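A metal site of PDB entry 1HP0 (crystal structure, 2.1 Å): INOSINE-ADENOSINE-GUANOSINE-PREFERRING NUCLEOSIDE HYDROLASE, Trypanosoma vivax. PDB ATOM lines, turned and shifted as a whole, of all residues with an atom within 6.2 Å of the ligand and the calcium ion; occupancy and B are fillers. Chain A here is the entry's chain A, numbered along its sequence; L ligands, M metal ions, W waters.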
ATOM      1  N   HIS A  21      15.828  19.257  30.031  1.00  0.00           N
ATOM      2  CA  HIS A  21      16.810  18.577  29.183  1.00  0.00           C
ATOM      3  C   HIS A  21      18.226  18.511  29.719  1.00  0.00           C
ATOM      4  O   HIS A  21      18.551  19.136  30.724  1.00  0.00           O
ATOM      5  CB  HIS A  21      16.830  19.267  27.815  1.00  0.00           C
ATOM      6  CG  HIS A  21      17.558  20.574  27.807  1.00  0.00           C
ATOM      7  ND1 HIS A  21      18.908  20.669  27.574  1.00  0.00           N
ATOM      8  CD2 HIS A  21      17.128  21.845  28.052  1.00  0.00           C
ATOM      9  CE1 HIS A  21      19.289  21.937  27.660  1.00  0.00           C
ATOM     10  NE2 HIS A  21      18.232  22.666  27.953  1.00  0.00           N
ATOM     11  N   ASP A  22      19.074  17.743  29.031  1.00  0.00           N
ATOM     12  CA  ASP A  22      20.463  17.659  29.456  1.00  0.00           C
ATOM     13  C   ASP A  22      21.458  18.146  28.396  1.00  0.00           C
ATOM     14  O   ASP A  22      22.599  17.690  28.313  1.00  0.00           O
ATOM     15  CB  ASP A  22      20.819  16.239  29.936  1.00  0.00           C
ATOM     16  CG  ASP A  22      20.688  15.208  28.855  1.00  0.00           C
ATOM     17  OD1 ASP A  22      21.200  14.096  29.064  1.00  0.00           O
ATOM     18  OD2 ASP A  22      20.082  15.511  27.820  1.00  0.00           O
ATOM     19  N   GLY A  23      20.992  19.066  27.560  1.00  0.00           N
ATOM     20  CA  GLY A  23      21.848  19.690  26.574  1.00  0.00           C
ATOM     21  C   GLY A  23      22.673  18.981  25.518  1.00  0.00           C
ATOM     22  O   GLY A  23      23.788  19.428  25.209  1.00  0.00           O
ATOM     23  N   ASN A  24      22.193  17.883  24.948  1.00  0.00           N
ATOM     24  CA  ASN A  24      22.957  17.301  23.878  1.00  0.00           C
ATOM     25  C   ASN A  24      22.336  17.860  22.599  1.00  0.00           C
ATOM     26  O   ASN A  24      21.474  18.734  22.666  1.00  0.00           O
ATOM     27  CB  ASN A  24      22.919  15.795  23.871  1.00  0.00           C
ATOM     28  CG  ASN A  24      24.215  15.231  23.376  1.00  0.00           C
ATOM     29  OD1 ASN A  24      25.144  15.017  24.163  1.00  0.00           O
ATOM     30  ND2 ASN A  24      24.328  15.052  22.050  1.00  0.00           N
ATOM     31  N   LEU A  25      22.790  17.401  21.430  1.00  0.00           N
ATOM     32  CA  LEU A  25      22.265  17.948  20.171  1.00  0.00           C
ATOM     33  C   LEU A  25      20.768  17.774  19.982  1.00  0.00           C
ATOM     34  O   LEU A  25      20.073  18.720  19.656  1.00  0.00           O
ATOM     35  CB  LEU A  25      23.017  17.363  18.970  1.00  0.00           C
ATOM     36  CG  LEU A  25      24.466  17.819  18.699  1.00  0.00           C
ATOM     37  CD1 LEU A  25      24.585  19.341  18.651  1.00  0.00           C
ATOM     38  CD2 LEU A  25      25.354  17.296  19.776  1.00  0.00           C
ATOM     39  N   ASP A  26      20.259  16.563  20.195  1.00  0.00           N
ATOM     40  CA  ASP A  26      18.830  16.364  20.020  1.00  0.00           C
ATOM     41  C   ASP A  26      17.987  17.113  21.064  1.00  0.00           C
ATOM     42  O   ASP A  26      16.827  17.411  20.814  1.00  0.00           O
ATOM     43  CB  ASP A  26      18.499  14.852  19.978  1.00  0.00           C
ATOM     44  CG  ASP A  26      18.866  14.124  21.256  1.00  0.00           C
ATOM     45  OD1 ASP A  26      19.927  14.420  21.842  1.00  0.00           O
ATOM     46  OD2 ASP A  26      18.102  13.227  21.648  1.00  0.00           O
ATOM     47  N   ASP A  27      18.572  17.441  22.220  1.00  0.00           N
ATOM     48  CA  ASP A  27      17.856  18.207  23.241  1.00  0.00           C
ATOM     49  C   ASP A  27      17.580  19.598  22.670  1.00  0.00           C
ATOM     50  O   ASP A  27      16.518  20.148  22.861  1.00  0.00           O
ATOM     51  CB  ASP A  27      18.718  18.376  24.508  1.00  0.00           C
ATOM     52  CG  ASP A  27      18.919  17.086  25.249  1.00  0.00           C
ATOM     53  OD1 ASP A  27      18.117  16.784  26.150  1.00  0.00           O
ATOM     54  OD2 ASP A  27      19.874  16.373  24.905  1.00  0.00           O
ATOM     55  N   ASP A  52      24.110  14.645  29.975  1.00  0.00           N
ATOM     56  CA  ASP A  52      24.778  14.437  28.701  1.00  0.00           C
ATOM     57  C   ASP A  52      25.392  15.743  28.171  1.00  0.00           C
ATOM     58  O   ASP A  52      25.491  15.955  26.946  1.00  0.00           O
ATOM     59  CB  ASP A  52      23.815  13.870  27.663  1.00  0.00           C
ATOM     60  CG  ASP A  52      24.526  13.148  26.535  1.00  0.00           C
ATOM     61  OD1 ASP A  52      23.860  12.756  25.563  1.00  0.00           O
ATOM     62  OD2 ASP A  52      25.758  12.952  26.630  1.00  0.00           O
ATOM     63  N   PHE A  91      27.245   9.909  31.743  1.00  0.00           N
ATOM     64  CA  PHE A  91      27.347   9.716  30.295  1.00  0.00           C
ATOM     65  C   PHE A  91      28.832   9.726  29.902  1.00  0.00           C
ATOM     66  O   PHE A  91      29.674  10.305  30.616  1.00  0.00           O
ATOM     67  CB  PHE A  91      26.659  10.875  29.541  1.00  0.00           C
ATOM     68  CG  PHE A  91      25.157  10.743  29.409  1.00  0.00           C
ATOM     69  CD1 PHE A  91      24.302  11.098  30.440  1.00  0.00           C
ATOM     70  CD2 PHE A  91      24.604  10.263  28.209  1.00  0.00           C
ATOM     71  CE1 PHE A  91      22.911  10.978  30.308  1.00  0.00           C
ATOM     72  CE2 PHE A  91      23.218  10.147  28.056  1.00  0.00           C
ATOM     73  CZ  PHE A  91      22.368  10.499  29.106  1.00  0.00           C
ATOM     74  N   TRP A  95      30.522  12.377  24.561  1.00  0.00           N
ATOM     75  CA  TRP A  95      29.275  12.950  24.083  1.00  0.00           C
ATOM     76  C   TRP A  95      28.883  14.242  24.785  1.00  0.00           C
ATOM     77  O   TRP A  95      28.269  15.114  24.178  1.00  0.00           O
ATOM     78  CB  TRP A  95      28.102  11.979  24.260  1.00  0.00           C
ATOM     79  CG  TRP A  95      28.312  10.602  23.737  1.00  0.00           C
ATOM     80  CD1 TRP A  95      29.233  10.199  22.811  1.00  0.00           C
ATOM     81  CD2 TRP A  95      27.554   9.447  24.087  1.00  0.00           C
ATOM     82  NE1 TRP A  95      29.089   8.858  22.568  1.00  0.00           N
ATOM     83  CE2 TRP A  95      28.063   8.367  23.336  1.00  0.00           C
ATOM     84  CE3 TRP A  95      26.483   9.220  24.968  1.00  0.00           C
ATOM     85  CZ2 TRP A  95      27.533   7.069  23.430  1.00  0.00           C
ATOM     86  CZ3 TRP A  95      25.952   7.932  25.063  1.00  0.00           C
ATOM     87  CH2 TRP A  95      26.484   6.878  24.290  1.00  0.00           C
ATOM     88  N   THR A 149      13.772  15.388  28.251  1.00  0.00           N
ATOM     89  CA  THR A 149      14.676  14.799  27.266  1.00  0.00           C
ATOM     90  C   THR A 149      16.013  14.393  27.848  1.00  0.00           C
ATOM     91  O   THR A 149      16.924  13.952  27.125  1.00  0.00           O
ATOM     92  CB  THR A 149      14.904  15.739  26.091  1.00  0.00           C
ATOM     93  OG1 THR A 149      15.505  16.956  26.559  1.00  0.00           O
ATOM     94  CG2 THR A 149      13.590  16.060  25.402  1.00  0.00           C
ATOM     95  N   GLY A 150      16.145  14.560  29.155  1.00  0.00           N
ATOM     96  CA  GLY A 150      17.358  14.165  29.856  1.00  0.00           C
ATOM     97  C   GLY A 150      16.892  13.184  30.928  1.00  0.00           C
ATOM     98  O   GLY A 150      15.773  12.654  30.818  1.00  0.00           O
ATOM     99  N   PRO A 151      17.700  12.902  31.968  1.00  0.00           N
ATOM    100  CA  PRO A 151      17.297  11.961  33.022  1.00  0.00           C
ATOM    101  C   PRO A 151      16.100  12.441  33.837  1.00  0.00           C
ATOM    102  O   PRO A 151      15.738  13.612  33.821  1.00  0.00           O
ATOM    103  CB  PRO A 151      18.566  11.815  33.875  1.00  0.00           C
ATOM    104  CG  PRO A 151      19.676  12.043  32.864  1.00  0.00           C
ATOM    105  CD  PRO A 151      19.138  13.226  32.053  1.00  0.00           C
ATOM    106  N   MET A 176      11.510  11.076  27.158  1.00  0.00           N
ATOM    107  CA  MET A 176      12.338  10.332  26.209  1.00  0.00           C
ATOM    108  C   MET A 176      13.191   9.445  27.107  1.00  0.00           C
ATOM    109  O   MET A 176      13.964   9.938  27.947  1.00  0.00           O
ATOM    110  CB  MET A 176      13.249  11.244  25.390  1.00  0.00           C
ATOM    111  CG  MET A 176      14.039  10.497  24.285  1.00  0.00           C
ATOM    112  SD  MET A 176      15.371   9.423  24.922  1.00  0.00           S
ATOM    113  CE  MET A 176      15.019   7.823  24.186  1.00  0.00           C
ATOM    114  N   ASN A 185      20.646   0.963  24.753  1.00  0.00           N
ATOM    115  CA  ASN A 185      21.784   1.557  24.056  1.00  0.00           C
ATOM    116  C   ASN A 185      22.929   1.871  25.008  1.00  0.00           C
ATOM    117  O   ASN A 185      23.846   2.615  24.670  1.00  0.00           O
ATOM    118  CB  ASN A 185      21.393   2.804  23.255  1.00  0.00           C
ATOM    119  CG  ASN A 185      20.795   3.931  24.111  1.00  0.00           C
ATOM    120  OD1 ASN A 185      20.769   3.859  25.339  1.00  0.00           O
ATOM    121  ND2 ASN A 185      20.329   4.981  23.434  1.00  0.00           N
ATOM    122  N   GLU A 196      18.638   1.939  28.596  1.00  0.00           N
ATOM    123  CA  GLU A 196      18.772   3.135  27.768  1.00  0.00           C
ATOM    124  C   GLU A 196      19.432   4.195  28.677  1.00  0.00           C
ATOM    125  O   GLU A 196      19.175   4.213  29.879  1.00  0.00           O
ATOM    126  CB  GLU A 196      17.392   3.586  27.261  1.00  0.00           C
ATOM    127  CG  GLU A 196      17.406   4.876  26.467  1.00  0.00           C
ATOM    128  CD  GLU A 196      17.405   6.112  27.363  1.00  0.00           C
ATOM    129  OE1 GLU A 196      17.996   7.145  26.959  1.00  0.00           O
ATOM    130  OE2 GLU A 196      16.813   6.038  28.455  1.00  0.00           O
ATOM    131  N   TRP A 197      20.258   5.055  28.094  1.00  0.00           N
ATOM    132  CA  TRP A 197      20.996   6.075  28.840  1.00  0.00           C
ATOM    133  C   TRP A 197      20.316   7.010  29.843  1.00  0.00           C
ATOM    134  O   TRP A 197      20.812   7.119  30.969  1.00  0.00           O
ATOM    135  CB  TRP A 197      21.859   6.920  27.879  1.00  0.00           C
ATOM    136  CG  TRP A 197      23.131   6.237  27.559  1.00  0.00           C
ATOM    137  CD1 TRP A 197      23.424   5.521  26.442  1.00  0.00           C
ATOM    138  CD2 TRP A 197      24.266   6.116  28.420  1.00  0.00           C
ATOM    139  NE1 TRP A 197      24.665   4.957  26.552  1.00  0.00           N
ATOM    140  CE2 TRP A 197      25.206   5.303  27.759  1.00  0.00           C
ATOM    141  CE3 TRP A 197      24.576   6.600  29.699  1.00  0.00           C
ATOM    142  CZ2 TRP A 197      26.438   4.961  28.319  1.00  0.00           C
ATOM    143  CZ3 TRP A 197      25.817   6.269  30.257  1.00  0.00           C
ATOM    144  CH2 TRP A 197      26.721   5.457  29.563  1.00  0.00           C
ATOM    145  N   ASN A 198      19.236   7.698  29.470  1.00  0.00           N
ATOM    146  CA  ASN A 198      18.595   8.592  30.430  1.00  0.00           C
ATOM    147  C   ASN A 198      18.140   7.897  31.719  1.00  0.00           C
ATOM    148  O   ASN A 198      18.263   8.459  32.808  1.00  0.00           O
ATOM    149  CB  ASN A 198      17.393   9.323  29.808  1.00  0.00           C
ATOM    150  CG  ASN A 198      17.795  10.300  28.717  1.00  0.00           C
ATOM    151  OD1 ASN A 198      18.943  10.765  28.660  1.00  0.00           O
ATOM    152  ND2 ASN A 198      16.848  10.624  27.853  1.00  0.00           N
ATOM    153  N   LEU A 222      13.305   3.571  23.228  1.00  0.00           N
ATOM    154  CA  LEU A 222      13.963   3.238  21.972  1.00  0.00           C
ATOM    155  C   LEU A 222      13.026   2.526  20.973  1.00  0.00           C
ATOM    156  O   LEU A 222      13.294   2.499  19.769  1.00  0.00           O
ATOM    157  CB  LEU A 222      15.243   2.434  22.231  1.00  0.00           C
ATOM    158  CG  LEU A 222      16.249   3.134  23.153  1.00  0.00           C
ATOM    159  CD1 LEU A 222      17.552   2.374  23.116  1.00  0.00           C
ATOM    160  CD2 LEU A 222      16.480   4.618  22.730  1.00  0.00           C
ATOM    161  N   GLY A 268      23.219   4.921  14.131  1.00  0.00           N
ATOM    162  CA  GLY A 268      24.156   5.258  15.198  1.00  0.00           C
ATOM    163  C   GLY A 268      23.702   6.468  16.005  1.00  0.00           C
ATOM    164  O   GLY A 268      24.040   6.603  17.185  1.00  0.00           O
ATOM    165  N   TYR A 269      22.935   7.341  15.345  1.00  0.00           N
ATOM    166  CA  TYR A 269      22.405   8.559  15.963  1.00  0.00           C
ATOM    167  C   TYR A 269      20.918   8.739  15.578  1.00  0.00           C
ATOM    168  O   TYR A 269      20.561   8.743  14.397  1.00  0.00           O
ATOM    169  CB  TYR A 269      23.206   9.775  15.499  1.00  0.00           C
ATOM    170  CG  TYR A 269      24.315  10.189  16.439  1.00  0.00           C
ATOM    171  CD1 TYR A 269      25.409   9.349  16.668  1.00  0.00           C
ATOM    172  CD2 TYR A 269      24.266  11.409  17.116  1.00  0.00           C
ATOM    173  CE1 TYR A 269      26.433   9.720  17.558  1.00  0.00           C
ATOM    174  CE2 TYR A 269      25.287  11.790  17.997  1.00  0.00           C
ATOM    175  CZ  TYR A 269      26.361  10.940  18.220  1.00  0.00           C
ATOM    176  OH  TYR A 269      27.365  11.308  19.113  1.00  0.00           O
ATOM    177  N   TRP A 272      16.144  11.160  18.883  1.00  0.00           N
ATOM    178  CA  TRP A 272      15.484  10.813  20.141  1.00  0.00           C
ATOM    179  C   TRP A 272      14.633  11.904  20.765  1.00  0.00           C
ATOM    180  O   TRP A 272      13.403  11.799  20.799  1.00  0.00           O
ATOM    181  CB  TRP A 272      16.522  10.351  21.186  1.00  0.00           C
ATOM    182  CG  TRP A 272      17.498   9.277  20.754  1.00  0.00           C
ATOM    183  CD1 TRP A 272      17.303   7.929  20.735  1.00  0.00           C
ATOM    184  CD2 TRP A 272      18.877   9.487  20.375  1.00  0.00           C
ATOM    185  NE1 TRP A 272      18.462   7.279  20.380  1.00  0.00           N
ATOM    186  CE2 TRP A 272      19.446   8.208  20.153  1.00  0.00           C
ATOM    187  CE3 TRP A 272      19.674  10.619  20.220  1.00  0.00           C
ATOM    188  CZ2 TRP A 272      20.796   8.037  19.786  1.00  0.00           C
ATOM    189  CZ3 TRP A 272      21.033  10.449  19.852  1.00  0.00           C
ATOM    190  CH2 TRP A 272      21.565   9.164  19.646  1.00  0.00           C
ATOM    191  N   ASP A 273      15.284  12.948  21.274  1.00  0.00           N
ATOM    192  CA  ASP A 273      14.584  14.040  21.941  1.00  0.00           C
ATOM    193  C   ASP A 273      13.676  14.862  21.027  1.00  0.00           C
ATOM    194  O   ASP A 273      12.634  15.342  21.452  1.00  0.00           O
ATOM    195  CB  ASP A 273      15.596  14.988  22.615  1.00  0.00           C
ATOM    196  CG  ASP A 273      16.451  14.274  23.655  1.00  0.00           C
ATOM    197  OD1 ASP A 273      16.045  13.198  24.140  1.00  0.00           O
ATOM    198  OD2 ASP A 273      17.537  14.791  23.975  1.00  0.00           O
HETATM  199  O1  LIG L   1      19.302   7.602  24.819  1.00  0.00           O
HETATM  200  C1  LIG L   1      18.873   8.893  24.409  1.00  0.00           C
HETATM  201  C2  LIG L   1      19.259  10.036  25.393  1.00  0.00           C
HETATM  202  O2  LIG L   1      20.711   9.936  25.250  1.00  0.00           O
HETATM  203  C3  LIG L   1      18.762  11.184  24.498  1.00  0.00           C
HETATM  204  O3  LIG L   1      17.955  12.006  25.338  1.00  0.00           O
HETATM  205  C4  LIG L   1      20.044  11.840  23.904  1.00  0.00           C
HETATM  206  O4  LIG L   1      20.258  13.234  24.119  1.00  0.00           O
HETATM  207  C5  LIG L   1      21.209  11.039  24.493  1.00  0.00           C
HETATM  208  N1  LIG L   1      22.386  10.760  23.604  1.00  0.00           N
HETATM  209  C6  LIG L   1      23.211  11.718  22.971  1.00  0.00           C
HETATM  210  N2  LIG L   1      24.176  11.225  22.221  1.00  0.00           N
HETATM  211  C7  LIG L   1      23.992   9.838  22.349  1.00  0.00           C
HETATM  212  C8  LIG L   1      24.698   8.691  21.787  1.00  0.00           C
HETATM  213  N3  LIG L   1      25.736   8.794  20.970  1.00  0.00           N
HETATM  214  N4  LIG L   1      24.239   7.428  22.127  1.00  0.00           N
HETATM  215  C9  LIG L   1      23.167   7.289  22.957  1.00  0.00           C
HETATM  216  C10 LIG L   1      22.430   8.254  23.554  1.00  0.00           C
HETATM  217  C11 LIG L   1      22.894   9.532  23.195  1.00  0.00           C
HETATM  218 CA    CA M   1      18.883  14.320  25.984  1.00  0.00          CA
HETATM  219  O   HOH W   1      20.304  12.634  27.291  1.00  0.00           O
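A nitrogen (N1) of the ligand lies close to the side-chain carboxylate (OD1) of Asp 52, 3.2 Å away.
ND2 of Asn 24 touches C6 of the ligand (3.6 Å).
Phe 91 touches the ligand.
Trp 95 touches the ligand (CH2 to N4, 3.2 Å).
CD1 of Trp 197 touches C9 of the ligand, at 3.9 Å.
Tyr 269 touches the ligand.
Trp 272 touches the ligand.
Hydrophobic or aromatic side chains that line the ligand: Phe 91, Trp 95, Met 176, Trp 197, Tyr 269 and Trp 272.
15 residues have an atom within 4 Å of the ligand: Asn 24, Asp 26, Asp 27, Asp 52, Phe 91, Trp 95, Thr 149, Met 176, Asn 185, Glu 196, Trp 197, Asn 198, Tyr 269, Trp 272 and Asp 273.
Along chain A the residues within 4 Å of the calcium ion span positions 22 to 273.
The nearest printed residue that does not touch the calcium ion is Gly 150 (4.2 Å).
ND2 of Asn 198 sits close to O3 of the ligand (3.1 Å).
SD of Met 176 sits close to O3 of the ligand.
OD1 of Asp 26 lies close to O4 of the ligand (2.6 Å).
The side-chain amide nitrogen (ND2) of Asn 185 sits at hydrogen-bond distance from an oxygen (O1) of the ligand (3.1 Å).
OE1 of Glu 196 lies within hydrogen-bond range of O1 of the ligand, 2.5 Å away.
The calcium ion is bound by O of Thr 149 (2.3 Å).
OD2 of Asp 273 binds the calcium ion (2.5 Å).
OD2 of Asp 22 binds the calcium ion (2.5 Å).
The calcium ion is bound by the side-chain carboxylate (OD2) of Asp 27, at 2.5 Å.
The calcium ion is bound by O4 of the ligand.
The calcium ion is bound by water W1 (2.6 Å).
O3 of the ligand binds the calcium ion.
The calcium ion is bound by OD1 of Asp 27.
The calcium ion has eight donor atoms within binding distance.
O of Thr 149 sits close to ND2 of Asn 198, 3.4 Å away.
OD2 of Asp 27 sits close to N of Asn 24, at 2.8 Å.
The backbone NH of Asn 198 is in hydrogen-bond range of the side-chain carboxylate of Glu 196.
The side-chain amide oxygen of Asn 24 sits close to the side-chain carboxylate of Asp 52, at 3.0 Å.
The side-chain amide oxygen (OD1) of Asn 185 is in hydrogen-bond range of the backbone NH (N) of Trp 197 (3.0 Å).
The side-chain amide nitrogen of Asn 198 is in hydrogen-bond range of the backbone carbonyl oxygen of Met 176 (3.0 Å).
The side-chain carboxylate of Asp 26 lies close to the backbone NH of Asp 273 (2.9 Å).
The side-chain amide oxygen of Asn 24 lies close to the backbone carbonyl oxygen of Trp 95 (3.1 Å).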
